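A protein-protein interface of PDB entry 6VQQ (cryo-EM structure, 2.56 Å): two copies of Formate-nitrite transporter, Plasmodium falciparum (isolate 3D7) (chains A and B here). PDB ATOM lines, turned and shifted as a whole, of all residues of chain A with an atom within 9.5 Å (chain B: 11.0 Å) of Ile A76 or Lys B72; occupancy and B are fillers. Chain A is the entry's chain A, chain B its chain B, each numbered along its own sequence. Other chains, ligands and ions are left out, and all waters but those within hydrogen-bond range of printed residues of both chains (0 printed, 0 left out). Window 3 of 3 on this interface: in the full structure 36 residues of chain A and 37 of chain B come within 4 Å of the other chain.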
ATOM      1  N   TYR A  70       9.709  34.111 -23.630  1.00  0.00           N
ATOM      2  CA  TYR A  70       9.145  35.327 -24.201  1.00  0.00           C
ATOM      3  C   TYR A  70       7.627  35.350 -24.108  1.00  0.00           C
ATOM      4  O   TYR A  70       6.988  34.314 -23.909  1.00  0.00           O
ATOM      5  CB  TYR A  70       9.590  35.465 -25.659  1.00  0.00           C
ATOM      6  CG  TYR A  70       9.625  36.881 -26.188  1.00  0.00           C
ATOM      7  CD1 TYR A  70      10.749  37.670 -26.028  1.00  0.00           C
ATOM      8  CD2 TYR A  70       8.541  37.419 -26.863  1.00  0.00           C
ATOM      9  CE1 TYR A  70      10.790  38.957 -26.512  1.00  0.00           C
ATOM     10  CE2 TYR A  70       8.569  38.705 -27.350  1.00  0.00           C
ATOM     11  CZ  TYR A  70       9.698  39.471 -27.174  1.00  0.00           C
ATOM     12  OH  TYR A  70       9.738  40.760 -27.658  1.00  0.00           O
ATOM     13  N   HIS A  71       7.056  36.545 -24.240  1.00  0.00           N
ATOM     14  CA  HIS A  71       5.611  36.727 -24.188  1.00  0.00           C
ATOM     15  C   HIS A  71       4.891  35.794 -25.152  1.00  0.00           C
ATOM     16  O   HIS A  71       3.975  35.061 -24.764  1.00  0.00           O
ATOM     17  CB  HIS A  71       5.288  38.185 -24.502  1.00  0.00           C
ATOM     18  CG  HIS A  71       3.844  38.535 -24.353  1.00  0.00           C
ATOM     19  ND1 HIS A  71       3.303  39.686 -24.885  1.00  0.00           N
ATOM     20  CD2 HIS A  71       2.829  37.895 -23.728  1.00  0.00           C
ATOM     21  CE1 HIS A  71       2.016  39.737 -24.596  1.00  0.00           C
ATOM     22  NE2 HIS A  71       1.702  38.662 -23.896  1.00  0.00           N
ATOM     23  N   LYS A  72       5.299  35.810 -26.422  1.00  0.00           N
ATOM     24  CA  LYS A  72       4.533  35.120 -27.455  1.00  0.00           C
ATOM     25  C   LYS A  72       4.837  33.629 -27.467  1.00  0.00           C
ATOM     26  O   LYS A  72       3.959  32.810 -27.760  1.00  0.00           O
ATOM     27  CB  LYS A  72       4.833  35.738 -28.815  1.00  0.00           C
ATOM     28  CG  LYS A  72       4.561  37.227 -28.893  1.00  0.00           C
ATOM     29  CD  LYS A  72       3.105  37.543 -28.656  1.00  0.00           C
ATOM     30  CE  LYS A  72       2.760  38.938 -29.127  1.00  0.00           C
ATOM     31  NZ  LYS A  72       1.291  39.156 -29.179  1.00  0.00           N
ATOM     32  N   LEU A  73       6.078  33.260 -27.162  1.00  0.00           N
ATOM     33  CA  LEU A  73       6.433  31.848 -27.108  1.00  0.00           C
ATOM     34  C   LEU A  73       5.731  31.144 -25.955  1.00  0.00           C
ATOM     35  O   LEU A  73       5.610  29.915 -25.948  1.00  0.00           O
ATOM     36  CB  LEU A  73       7.947  31.710 -26.991  1.00  0.00           C
ATOM     37  CG  LEU A  73       8.544  30.315 -27.125  1.00  0.00           C
ATOM     38  CD1 LEU A  73       8.201  29.727 -28.468  1.00  0.00           C
ATOM     39  CD2 LEU A  73      10.047  30.364 -26.936  1.00  0.00           C
ATOM     40  N   ARG A  74       5.261  31.907 -24.965  1.00  0.00           N
ATOM     41  CA  ARG A  74       4.489  31.314 -23.879  1.00  0.00           C
ATOM     42  C   ARG A  74       3.099  30.906 -24.336  1.00  0.00           C
ATOM     43  O   ARG A  74       2.583  29.868 -23.906  1.00  0.00           O
ATOM     44  CB  ARG A  74       4.363  32.292 -22.717  1.00  0.00           C
ATOM     45  CG  ARG A  74       5.303  32.043 -21.555  1.00  0.00           C
ATOM     46  CD  ARG A  74       4.801  32.757 -20.328  1.00  0.00           C
ATOM     47  NE  ARG A  74       5.148  34.170 -20.342  1.00  0.00           N
ATOM     48  CZ  ARG A  74       4.600  35.080 -19.547  1.00  0.00           C
ATOM     49  NH1 ARG A  74       3.665  34.730 -18.670  1.00  0.00           N
ATOM     50  NH2 ARG A  74       4.985  36.341 -19.637  1.00  0.00           N
ATOM     51  N   GLU A  75       2.476  31.710 -25.190  1.00  0.00           N
ATOM     52  CA  GLU A  75       1.119  31.467 -25.649  1.00  0.00           C
ATOM     53  C   GLU A  75       1.024  30.314 -26.639  1.00  0.00           C
ATOM     54  O   GLU A  75      -0.047  30.103 -27.215  1.00  0.00           O
ATOM     55  CB  GLU A  75       0.553  32.739 -26.279  1.00  0.00           C
ATOM     56  CG  GLU A  75      -0.952  32.847 -26.196  1.00  0.00           C
ATOM     57  CD  GLU A  75      -1.470  34.178 -26.701  1.00  0.00           C
ATOM     58  OE1 GLU A  75      -1.331  35.186 -25.977  1.00  0.00           O
ATOM     59  OE2 GLU A  75      -2.019  34.217 -27.823  1.00  0.00           O
ATOM     60  N   ILE A  76       2.110  29.578 -26.857  1.00  0.00           N
ATOM     61  CA  ILE A  76       2.090  28.401 -27.714  1.00  0.00           C
ATOM     62  C   ILE A  76       2.625  27.206 -26.938  1.00  0.00           C
ATOM     63  O   ILE A  76       1.943  26.184 -26.814  1.00  0.00           O
ATOM     64  CB  ILE A  76       2.901  28.638 -29.000  1.00  0.00           C
ATOM     65  CG1 ILE A  76       2.360  29.855 -29.746  1.00  0.00           C
ATOM     66  CG2 ILE A  76       2.840  27.420 -29.908  1.00  0.00           C
ATOM     67  CD1 ILE A  76       3.229  30.292 -30.893  1.00  0.00           C
ATOM     68  N   VAL A  77       3.844  27.324 -26.406  1.00  0.00           N
ATOM     69  CA  VAL A  77       4.503  26.203 -25.748  1.00  0.00           C
ATOM     70  C   VAL A  77       4.539  26.342 -24.233  1.00  0.00           C
ATOM     71  O   VAL A  77       5.158  25.506 -23.561  1.00  0.00           O
ATOM     72  CB  VAL A  77       5.928  26.004 -26.302  1.00  0.00           C
ATOM     73  CG1 VAL A  77       5.876  25.830 -27.807  1.00  0.00           C
ATOM     74  CG2 VAL A  77       6.832  27.165 -25.938  1.00  0.00           C
ATOM     75  N   GLY A  78       3.891  27.358 -23.673  1.00  0.00           N
ATOM     76  CA  GLY A  78       3.879  27.545 -22.237  1.00  0.00           C
ATOM     77  C   GLY A  78       5.258  27.603 -21.614  1.00  0.00           C
ATOM     78  O   GLY A  78       6.018  28.545 -21.860  1.00  0.00           O
ATOM     79  N   ALA A  79       5.596  26.596 -20.806  1.00  0.00           N
ATOM     80  CA  ALA A  79       6.849  26.556 -20.063  1.00  0.00           C
ATOM     81  C   ALA A  79       7.702  25.359 -20.459  1.00  0.00           C
ATOM     82  O   ALA A  79       8.414  24.792 -19.629  1.00  0.00           O
ATOM     83  CB  ALA A  79       6.580  26.533 -18.561  1.00  0.00           C
ATOM     84  N   SER A  80       7.646  24.974 -21.731  1.00  0.00           N
ATOM     85  CA  SER A  80       8.285  23.743 -22.180  1.00  0.00           C
ATOM     86  C   SER A  80       9.778  23.927 -22.422  1.00  0.00           C
ATOM     87  O   SER A  80      10.609  23.281 -21.777  1.00  0.00           O
ATOM     88  CB  SER A  80       7.596  23.254 -23.451  1.00  0.00           C
ATOM     89  OG  SER A  80       8.213  22.086 -23.950  1.00  0.00           O
ATOM     90  N   MET A  81      10.136  24.803 -23.361  1.00  0.00           N
ATOM     91  CA  MET A  81      11.530  24.934 -23.761  1.00  0.00           C
ATOM     92  C   MET A  81      12.399  25.451 -22.622  1.00  0.00           C
ATOM     93  O   MET A  81      13.579  25.088 -22.524  1.00  0.00           O
ATOM     94  CB  MET A  81      11.634  25.866 -24.965  1.00  0.00           C
ATOM     95  CG  MET A  81      10.824  25.431 -26.172  1.00  0.00           C
ATOM     96  SD  MET A  81      11.243  23.782 -26.759  1.00  0.00           S
ATOM     97  CE  MET A  81      12.955  24.018 -27.212  1.00  0.00           C
ATOM     98  N   GLY B  65       7.620  14.867 -21.015  1.00  0.00           N
ATOM     99  CA  GLY B  65       6.707  14.753 -22.138  1.00  0.00           C
ATOM    100  C   GLY B  65       5.432  15.548 -21.952  1.00  0.00           C
ATOM    101  O   GLY B  65       4.928  16.157 -22.897  1.00  0.00           O
ATOM    102  N   GLY B  66       4.886  15.551 -20.737  1.00  0.00           N
ATOM    103  CA  GLY B  66       3.678  16.315 -20.498  1.00  0.00           C
ATOM    104  C   GLY B  66       3.934  17.805 -20.515  1.00  0.00           C
ATOM    105  O   GLY B  66       3.095  18.585 -20.971  1.00  0.00           O
ATOM    106  N   LEU B  67       5.095  18.220 -20.016  1.00  0.00           N
ATOM    107  CA  LEU B  67       5.514  19.604 -20.172  1.00  0.00           C
ATOM    108  C   LEU B  67       5.515  19.993 -21.639  1.00  0.00           C
ATOM    109  O   LEU B  67       5.136  21.114 -21.996  1.00  0.00           O
ATOM    110  CB  LEU B  67       6.900  19.777 -19.556  1.00  0.00           C
ATOM    111  CG  LEU B  67       7.425  21.152 -19.168  1.00  0.00           C
ATOM    112  CD1 LEU B  67       6.344  22.041 -18.587  1.00  0.00           C
ATOM    113  CD2 LEU B  67       8.543  20.944 -18.164  1.00  0.00           C
ATOM    114  N   PHE B  68       5.922  19.069 -22.507  1.00  0.00           N
ATOM    115  CA  PHE B  68       5.867  19.312 -23.941  1.00  0.00           C
ATOM    116  C   PHE B  68       4.496  19.027 -24.542  1.00  0.00           C
ATOM    117  O   PHE B  68       4.236  19.437 -25.677  1.00  0.00           O
ATOM    118  CB  PHE B  68       6.924  18.469 -24.649  1.00  0.00           C
ATOM    119  CG  PHE B  68       8.172  19.223 -24.966  1.00  0.00           C
ATOM    120  CD1 PHE B  68       8.253  19.998 -26.103  1.00  0.00           C
ATOM    121  CD2 PHE B  68       9.260  19.169 -24.122  1.00  0.00           C
ATOM    122  CE1 PHE B  68       9.400  20.701 -26.393  1.00  0.00           C
ATOM    123  CE2 PHE B  68      10.407  19.867 -24.407  1.00  0.00           C
ATOM    124  CZ  PHE B  68      10.478  20.634 -25.543  1.00  0.00           C
ATOM    125  N   TYR B  69       3.619  18.344 -23.816  1.00  0.00           N
ATOM    126  CA  TYR B  69       2.275  18.028 -24.299  1.00  0.00           C
ATOM    127  C   TYR B  69       1.271  19.095 -23.876  1.00  0.00           C
ATOM    128  O   TYR B  69       0.216  18.807 -23.317  1.00  0.00           O
ATOM    129  CB  TYR B  69       1.869  16.654 -23.782  1.00  0.00           C
ATOM    130  CG  TYR B  69       0.887  15.891 -24.642  1.00  0.00           C
ATOM    131  CD1 TYR B  69       1.114  15.698 -25.994  1.00  0.00           C
ATOM    132  CD2 TYR B  69      -0.253  15.337 -24.090  1.00  0.00           C
ATOM    133  CE1 TYR B  69       0.222  14.993 -26.771  1.00  0.00           C
ATOM    134  CE2 TYR B  69      -1.147  14.629 -24.858  1.00  0.00           C
ATOM    135  CZ  TYR B  69      -0.907  14.461 -26.196  1.00  0.00           C
ATOM    136  OH  TYR B  69      -1.807  13.757 -26.956  1.00  0.00           O
ATOM    137  N   TYR B  70       1.597  20.348 -24.167  1.00  0.00           N
ATOM    138  CA  TYR B  70       0.775  21.461 -23.721  1.00  0.00           C
ATOM    139  C   TYR B  70      -0.401  21.667 -24.670  1.00  0.00           C
ATOM    140  O   TYR B  70      -0.351  21.309 -25.849  1.00  0.00           O
ATOM    141  CB  TYR B  70       1.633  22.726 -23.601  1.00  0.00           C
ATOM    142  CG  TYR B  70       0.867  24.008 -23.357  1.00  0.00           C
ATOM    143  CD1 TYR B  70       0.316  24.284 -22.119  1.00  0.00           C
ATOM    144  CD2 TYR B  70       0.716  24.951 -24.358  1.00  0.00           C
ATOM    145  CE1 TYR B  70      -0.381  25.451 -21.891  1.00  0.00           C
ATOM    146  CE2 TYR B  70       0.021  26.120 -24.137  1.00  0.00           C
ATOM    147  CZ  TYR B  70      -0.525  26.364 -22.905  1.00  0.00           C
ATOM    148  OH  TYR B  70      -1.216  27.532 -22.698  1.00  0.00           O
ATOM    149  N   HIS B  71      -1.475  22.248 -24.132  1.00  0.00           N
ATOM    150  CA  HIS B  71      -2.750  22.307 -24.843  1.00  0.00           C
ATOM    151  C   HIS B  71      -2.595  22.886 -26.242  1.00  0.00           C
ATOM    152  O   HIS B  71      -3.175  22.372 -27.204  1.00  0.00           O
ATOM    153  CB  HIS B  71      -3.743  23.130 -24.026  1.00  0.00           C
ATOM    154  CG  HIS B  71      -4.970  23.530 -24.779  1.00  0.00           C
ATOM    155  ND1 HIS B  71      -5.655  22.666 -25.605  1.00  0.00           N
ATOM    156  CD2 HIS B  71      -5.644  24.702 -24.817  1.00  0.00           C
ATOM    157  CE1 HIS B  71      -6.693  23.293 -26.129  1.00  0.00           C
ATOM    158  NE2 HIS B  71      -6.708  24.529 -25.667  1.00  0.00           N
ATOM    159  N   LYS B  72      -1.811  23.955 -26.378  1.00  0.00           N
ATOM    160  CA  LYS B  72      -1.735  24.654 -27.655  1.00  0.00           C
ATOM    161  C   LYS B  72      -0.667  24.047 -28.555  1.00  0.00           C
ATOM    162  O   LYS B  72      -0.757  24.139 -29.785  1.00  0.00           O
ATOM    163  CB  LYS B  72      -1.452  26.135 -27.418  1.00  0.00           C
ATOM    164  CG  LYS B  72      -2.605  26.910 -26.821  1.00  0.00           C
ATOM    165  CD  LYS B  72      -3.835  26.874 -27.708  1.00  0.00           C
ATOM    166  CE  LYS B  72      -4.905  27.832 -27.219  1.00  0.00           C
ATOM    167  NZ  LYS B  72      -6.109  27.808 -28.086  1.00  0.00           N
ATOM    168  N   LEU B  73       0.348  23.420 -27.962  1.00  0.00           N
ATOM    169  CA  LEU B  73       1.408  22.815 -28.757  1.00  0.00           C
ATOM    170  C   LEU B  73       0.891  21.590 -29.501  1.00  0.00           C
ATOM    171  O   LEU B  73       1.317  21.308 -30.627  1.00  0.00           O
ATOM    172  CB  LEU B  73       2.569  22.438 -27.845  1.00  0.00           C
ATOM    173  CG  LEU B  73       3.954  22.200 -28.455  1.00  0.00           C
ATOM    174  CD1 LEU B  73       5.210  22.283 -27.567  1.00  0.00           C
ATOM    175  CD2 LEU B  73       4.120  21.502 -29.807  1.00  0.00           C
ATOM    176  N   ARG B  74      -0.033  20.850 -28.882  1.00  0.00           N
ATOM    177  CA  ARG B  74      -0.593  19.658 -29.509  1.00  0.00           C
ATOM    178  C   ARG B  74      -1.291  19.990 -30.820  1.00  0.00           C
ATOM    179  O   ARG B  74      -1.162  19.255 -31.805  1.00  0.00           O
ATOM    180  CB  ARG B  74      -1.575  18.983 -28.557  1.00  0.00           C
ATOM    181  CG  ARG B  74      -0.934  18.332 -27.368  1.00  0.00           C
ATOM    182  CD  ARG B  74      -1.938  17.532 -26.558  1.00  0.00           C
ATOM    183  NE  ARG B  74      -2.976  18.360 -25.961  1.00  0.00           N
ATOM    184  CZ  ARG B  74      -3.811  17.938 -25.017  1.00  0.00           C
ATOM    185  NH1 ARG B  74      -3.734  16.694 -24.571  1.00  0.00           N
ATOM    186  NH2 ARG B  74      -4.726  18.758 -24.521  1.00  0.00           N
ATOM    187  N   GLU B  75      -2.042  21.091 -30.851  1.00  0.00           N
ATOM    188  CA  GLU B  75      -2.858  21.395 -32.019  1.00  0.00           C
ATOM    189  C   GLU B  75      -2.002  21.630 -33.258  1.00  0.00           C
ATOM    190  O   GLU B  75      -2.526  21.723 -34.373  1.00  0.00           O
ATOM    191  CB  GLU B  75      -3.732  22.613 -31.738  1.00  0.00           C
ATOM    192  CG  GLU B  75      -5.043  22.288 -31.064  1.00  0.00           C
ATOM    193  CD  GLU B  75      -5.745  23.519 -30.529  1.00  0.00           C
ATOM    194  OE1 GLU B  75      -5.304  24.051 -29.488  1.00  0.00           O
ATOM    195  OE2 GLU B  75      -6.737  23.957 -31.149  1.00  0.00           O
ATOM    196  N   ILE B  76      -0.684  21.734 -33.083  1.00  0.00           N
ATOM    197  CA  ILE B  76       0.197  22.020 -34.206  1.00  0.00           C
ATOM    198  C   ILE B  76       1.149  20.860 -34.455  1.00  0.00           C
ATOM    199  O   ILE B  76       1.644  20.680 -35.572  1.00  0.00           O
ATOM    200  CB  ILE B  76       0.966  23.327 -33.949  1.00  0.00           C
ATOM    201  CG1 ILE B  76       0.005  24.494 -33.719  1.00  0.00           C
ATOM    202  CG2 ILE B  76       1.884  23.633 -35.113  1.00  0.00           C
ATOM    203  CD1 ILE B  76      -0.882  24.826 -34.900  1.00  0.00           C
ATOM    204  N   VAL B  77       1.423  20.059 -33.427  1.00  0.00           N
ATOM    205  CA  VAL B  77       2.482  19.062 -33.472  1.00  0.00           C
ATOM    206  C   VAL B  77       2.009  17.677 -33.062  1.00  0.00           C
ATOM    207  O   VAL B  77       2.661  16.687 -33.405  1.00  0.00           O
ATOM    208  CB  VAL B  77       3.674  19.501 -32.596  1.00  0.00           C
ATOM    209  CG1 VAL B  77       4.580  18.344 -32.286  1.00  0.00           C
ATOM    210  CG2 VAL B  77       4.440  20.617 -33.274  1.00  0.00           C
ATOM    211  N   GLY B  78       0.889  17.571 -32.361  1.00  0.00           N
ATOM    212  CA  GLY B  78       0.452  16.268 -31.897  1.00  0.00           C
ATOM    213  C   GLY B  78       1.242  15.834 -30.682  1.00  0.00           C
ATOM    214  O   GLY B  78       1.189  16.460 -29.619  1.00  0.00           O
ATOM    215  N   ALA B  79       1.990  14.742 -30.834  1.00  0.00           N
ATOM    216  CA  ALA B  79       2.743  14.145 -29.741  1.00  0.00           C
ATOM    217  C   ALA B  79       4.193  13.859 -30.103  1.00  0.00           C
ATOM    218  O   ALA B  79       4.785  12.929 -29.549  1.00  0.00           O
ATOM    219  CB  ALA B  79       2.065  12.855 -29.287  1.00  0.00           C
ATOM    220  N   MET B  81       7.207  15.971 -30.046  1.00  0.00           N
ATOM    221  CA  MET B  81       8.228  16.427 -29.113  1.00  0.00           C
ATOM    222  C   MET B  81       8.115  15.697 -27.784  1.00  0.00           C
ATOM    223  O   MET B  81       9.126  15.431 -27.123  1.00  0.00           O
ATOM    224  CB  MET B  81       8.108  17.936 -28.914  1.00  0.00           C
ATOM    225  CG  MET B  81       8.312  18.749 -30.178  1.00  0.00           C
ATOM    226  SD  MET B  81      10.004  18.653 -30.783  1.00  0.00           S
ATOM    227  CE  MET B  81      10.822  19.744 -29.627  1.00  0.00           C
ATOM    228  N   SER B  82       6.889  15.363 -27.378  1.00  0.00           N
ATOM    229  CA  SER B  82       6.685  14.604 -26.152  1.00  0.00           C
ATOM    230  C   SER B  82       7.497  13.319 -26.163  1.00  0.00           C
ATOM    231  O   SER B  82       8.341  13.088 -25.288  1.00  0.00           O
ATOM    232  CB  SER B  82       5.202  14.292 -25.979  1.00  0.00           C
ATOM    233  OG  SER B  82       4.446  15.465 -25.767  1.00  0.00           O
ATOM    234  N   ALA B 160      -8.663  21.054 -15.752  1.00  0.00           N
ATOM    235  CA  ALA B 160      -8.404  22.377 -16.310  1.00  0.00           C
ATOM    236  C   ALA B 160      -7.305  22.204 -17.340  1.00  0.00           C
ATOM    237  O   ALA B 160      -6.216  21.728 -17.005  1.00  0.00           O
ATOM    238  CB  ALA B 160      -7.995  23.366 -15.226  1.00  0.00           C
ATOM    239  N   VAL B 161      -7.580  22.590 -18.584  1.00  0.00           N
ATOM    240  CA  VAL B 161      -6.755  22.120 -19.691  1.00  0.00           C
ATOM    241  C   VAL B 161      -5.433  22.870 -19.736  1.00  0.00           C
ATOM    242  O   VAL B 161      -4.432  22.360 -20.254  1.00  0.00           O
ATOM    243  CB  VAL B 161      -7.529  22.243 -21.013  1.00  0.00           C
ATOM    244  CG1 VAL B 161      -6.777  21.550 -22.122  1.00  0.00           C
ATOM    245  CG2 VAL B 161      -8.919  21.656 -20.857  1.00  0.00           C
ATOM    246  N   GLU B 162      -5.399  24.082 -19.188  1.00  0.00           N
ATOM    247  CA  GLU B 162      -4.152  24.833 -19.153  1.00  0.00           C
ATOM    248  C   GLU B 162      -3.104  24.174 -18.268  1.00  0.00           C
ATOM    249  O   GLU B 162      -1.918  24.495 -18.394  1.00  0.00           O
ATOM    250  CB  GLU B 162      -4.409  26.259 -18.670  1.00  0.00           C
ATOM    251  CG  GLU B 162      -5.253  27.099 -19.613  1.00  0.00           C
ATOM    252  CD  GLU B 162      -6.741  26.908 -19.398  1.00  0.00           C
ATOM    253  OE1 GLU B 162      -7.118  26.163 -18.469  1.00  0.00           O
ATOM    254  OE2 GLU B 162      -7.534  27.504 -20.157  1.00  0.00           O
ATOM    255  N   LYS B 163      -3.509  23.261 -17.383  1.00  0.00           N
ATOM    256  CA  LYS B 163      -2.616  22.699 -16.380  1.00  0.00           C
ATOM    257  C   LYS B 163      -2.568  21.177 -16.387  1.00  0.00           C
ATOM    258  O   LYS B 163      -1.577  20.604 -15.926  1.00  0.00           O
ATOM    259  CB  LYS B 163      -3.039  23.159 -14.980  1.00  0.00           C
ATOM    260  CG  LYS B 163      -3.536  24.594 -14.883  1.00  0.00           C
ATOM    261  CD  LYS B 163      -2.401  25.574 -14.647  1.00  0.00           C
ATOM    262  CE  LYS B 163      -2.922  26.900 -14.124  1.00  0.00           C
ATOM    263  NZ  LYS B 163      -3.332  26.819 -12.696  1.00  0.00           N
ATOM    264  N   ASN B 164      -3.603  20.518 -16.899  1.00  0.00           N
ATOM    265  CA  ASN B 164      -3.758  19.074 -16.783  1.00  0.00           C
ATOM    266  C   ASN B 164      -2.861  18.284 -17.725  1.00  0.00           C
ATOM    267  O   ASN B 164      -3.061  17.074 -17.870  1.00  0.00           O
ATOM    268  CB  ASN B 164      -5.214  18.695 -17.050  1.00  0.00           C
ATOM    269  CG  ASN B 164      -5.670  17.514 -16.234  1.00  0.00           C
ATOM    270  OD1 ASN B 164      -4.969  17.051 -15.337  1.00  0.00           O
ATOM    271  ND2 ASN B 164      -6.857  17.019 -16.539  1.00  0.00           N
ATOM    272  N   HIS B 165      -1.878  18.918 -18.352  1.00  0.00           N
ATOM    273  CA  HIS B 165      -1.159  18.283 -19.449  1.00  0.00           C
ATOM    274  C   HIS B 165      -0.098  17.308 -18.959  1.00  0.00           C
ATOM    275  O   HIS B 165       0.627  16.720 -19.766  1.00  0.00           O
ATOM    276  CB  HIS B 165      -0.524  19.340 -20.359  1.00  0.00           C
ATOM    277  CG  HIS B 165       0.097  20.486 -19.627  1.00  0.00           C
ATOM    278  ND1 HIS B 165      -0.523  21.709 -19.506  1.00  0.00           N
ATOM    279  CD2 HIS B 165       1.280  20.597 -18.983  1.00  0.00           C
ATOM    280  CE1 HIS B 165       0.251  22.524 -18.814  1.00  0.00           C
ATOM    281  NE2 HIS B 165       1.351  21.874 -18.485  1.00  0.00           N
ATOM    282  N   GLN B 168      -3.304  14.202 -18.726  1.00  0.00           N
ATOM    283  CA  GLN B 168      -3.842  13.740 -19.999  1.00  0.00           C
ATOM    284  C   GLN B 168      -2.831  12.881 -20.743  1.00  0.00           C
ATOM    285  O   GLN B 168      -3.172  11.818 -21.274  1.00  0.00           O
ATOM    286  CB  GLN B 168      -4.264  14.937 -20.851  1.00  0.00           C
ATOM    287  CG  GLN B 168      -5.291  14.598 -21.900  1.00  0.00           C
ATOM    288  CD  GLN B 168      -6.680  14.462 -21.327  1.00  0.00           C
ATOM    289  OE1 GLN B 168      -7.162  15.344 -20.622  1.00  0.00           O
ATOM    290  NE2 GLN B 168      -7.332  13.347 -21.623  1.00  0.00           N
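CD2 of Tyr B70 touches O of Ile A76 (3.0 Å). O of Ile A76 touches CB of Lys B72, at 3.4 Å. Val A77 touches Leu B73 (CG1 to CD1, 3.6 Å). O of Ala A79 touches CD1 of Leu B67, 3.6 Å away. Ser A80 touches Leu B67 (CB to O, 3.6 Å). Ser A80 touches Phe B68. CZ of Phe B68 touches SD of Met A81, 3.5 Å away.
N of Leu B73 lies within hydrogen-bond range of O of Ile A76.
Ile A76 touches Tyr B70, but with the chains exchanged Tyr A70 does not touch Ile B76 (15.5 Å). Ile A76 touches Lys B72, but with the chains exchanged Lys A72 does not touch Ile B76 (11.0 Å). Ile A76 touches Leu B73, but with the chains exchanged Leu A73 does not touch Ile B76 (11.0 Å). Val A77 touches Leu B73, but with the chains exchanged Leu A73 does not touch Val B77 (11.0 Å). 11 positions are printed for both chains.
Ile A76 touches just these residues of chain B: Tyr B70, Lys B72 and Leu B73. Of chain B, only Leu B73 (3.6 Å) comes within 4 Å of Val A77. No residue of chain B comes within 4 Å of Gly A78. Of the printed residues of chain B, Ala A79 touches Leu B67. Of the printed residues of chain A, Leu B67 touches Ala A79 (3.6 Å) and Ser A80 (3.6 Å). Printed residues of chain A within 4 Å of Phe B68: Ser A80 (3.0 Å) and Met A81 (3.5 Å). Tyr B69 touches none of the printed residues of chain A. Of chain A, only Ile A76 (3.0 Å) comes within 4 Å of Tyr B70. No residue of chain A comes within 4 Å of His B71. The nearest residue of chain B that does not touch Ile A76 is Ile B76 (5.6 Å). The nearest residue of chain A that does not touch Lys B72 is Glu A75 (4.1 Å). The nearest printed residue of chain A that does not touch Leu B73 is Ser A80 (4.7 Å).
Printed residues of chain A that touch a printed residue of chain B: Ile A76, Val A77, Ala A79, Ser A80 and Met A81. Hydrophobic or aromatic side chains of chain A that line the printed part of chain B: Val A77 and Met A81. Hydrophobic or aromatic side chains of chain B within 4 Å of the printed part of chain A: Leu B67, Phe B68, Tyr B70 and Leu B73. Among the printed residues, 8 pairs touch across the chains.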
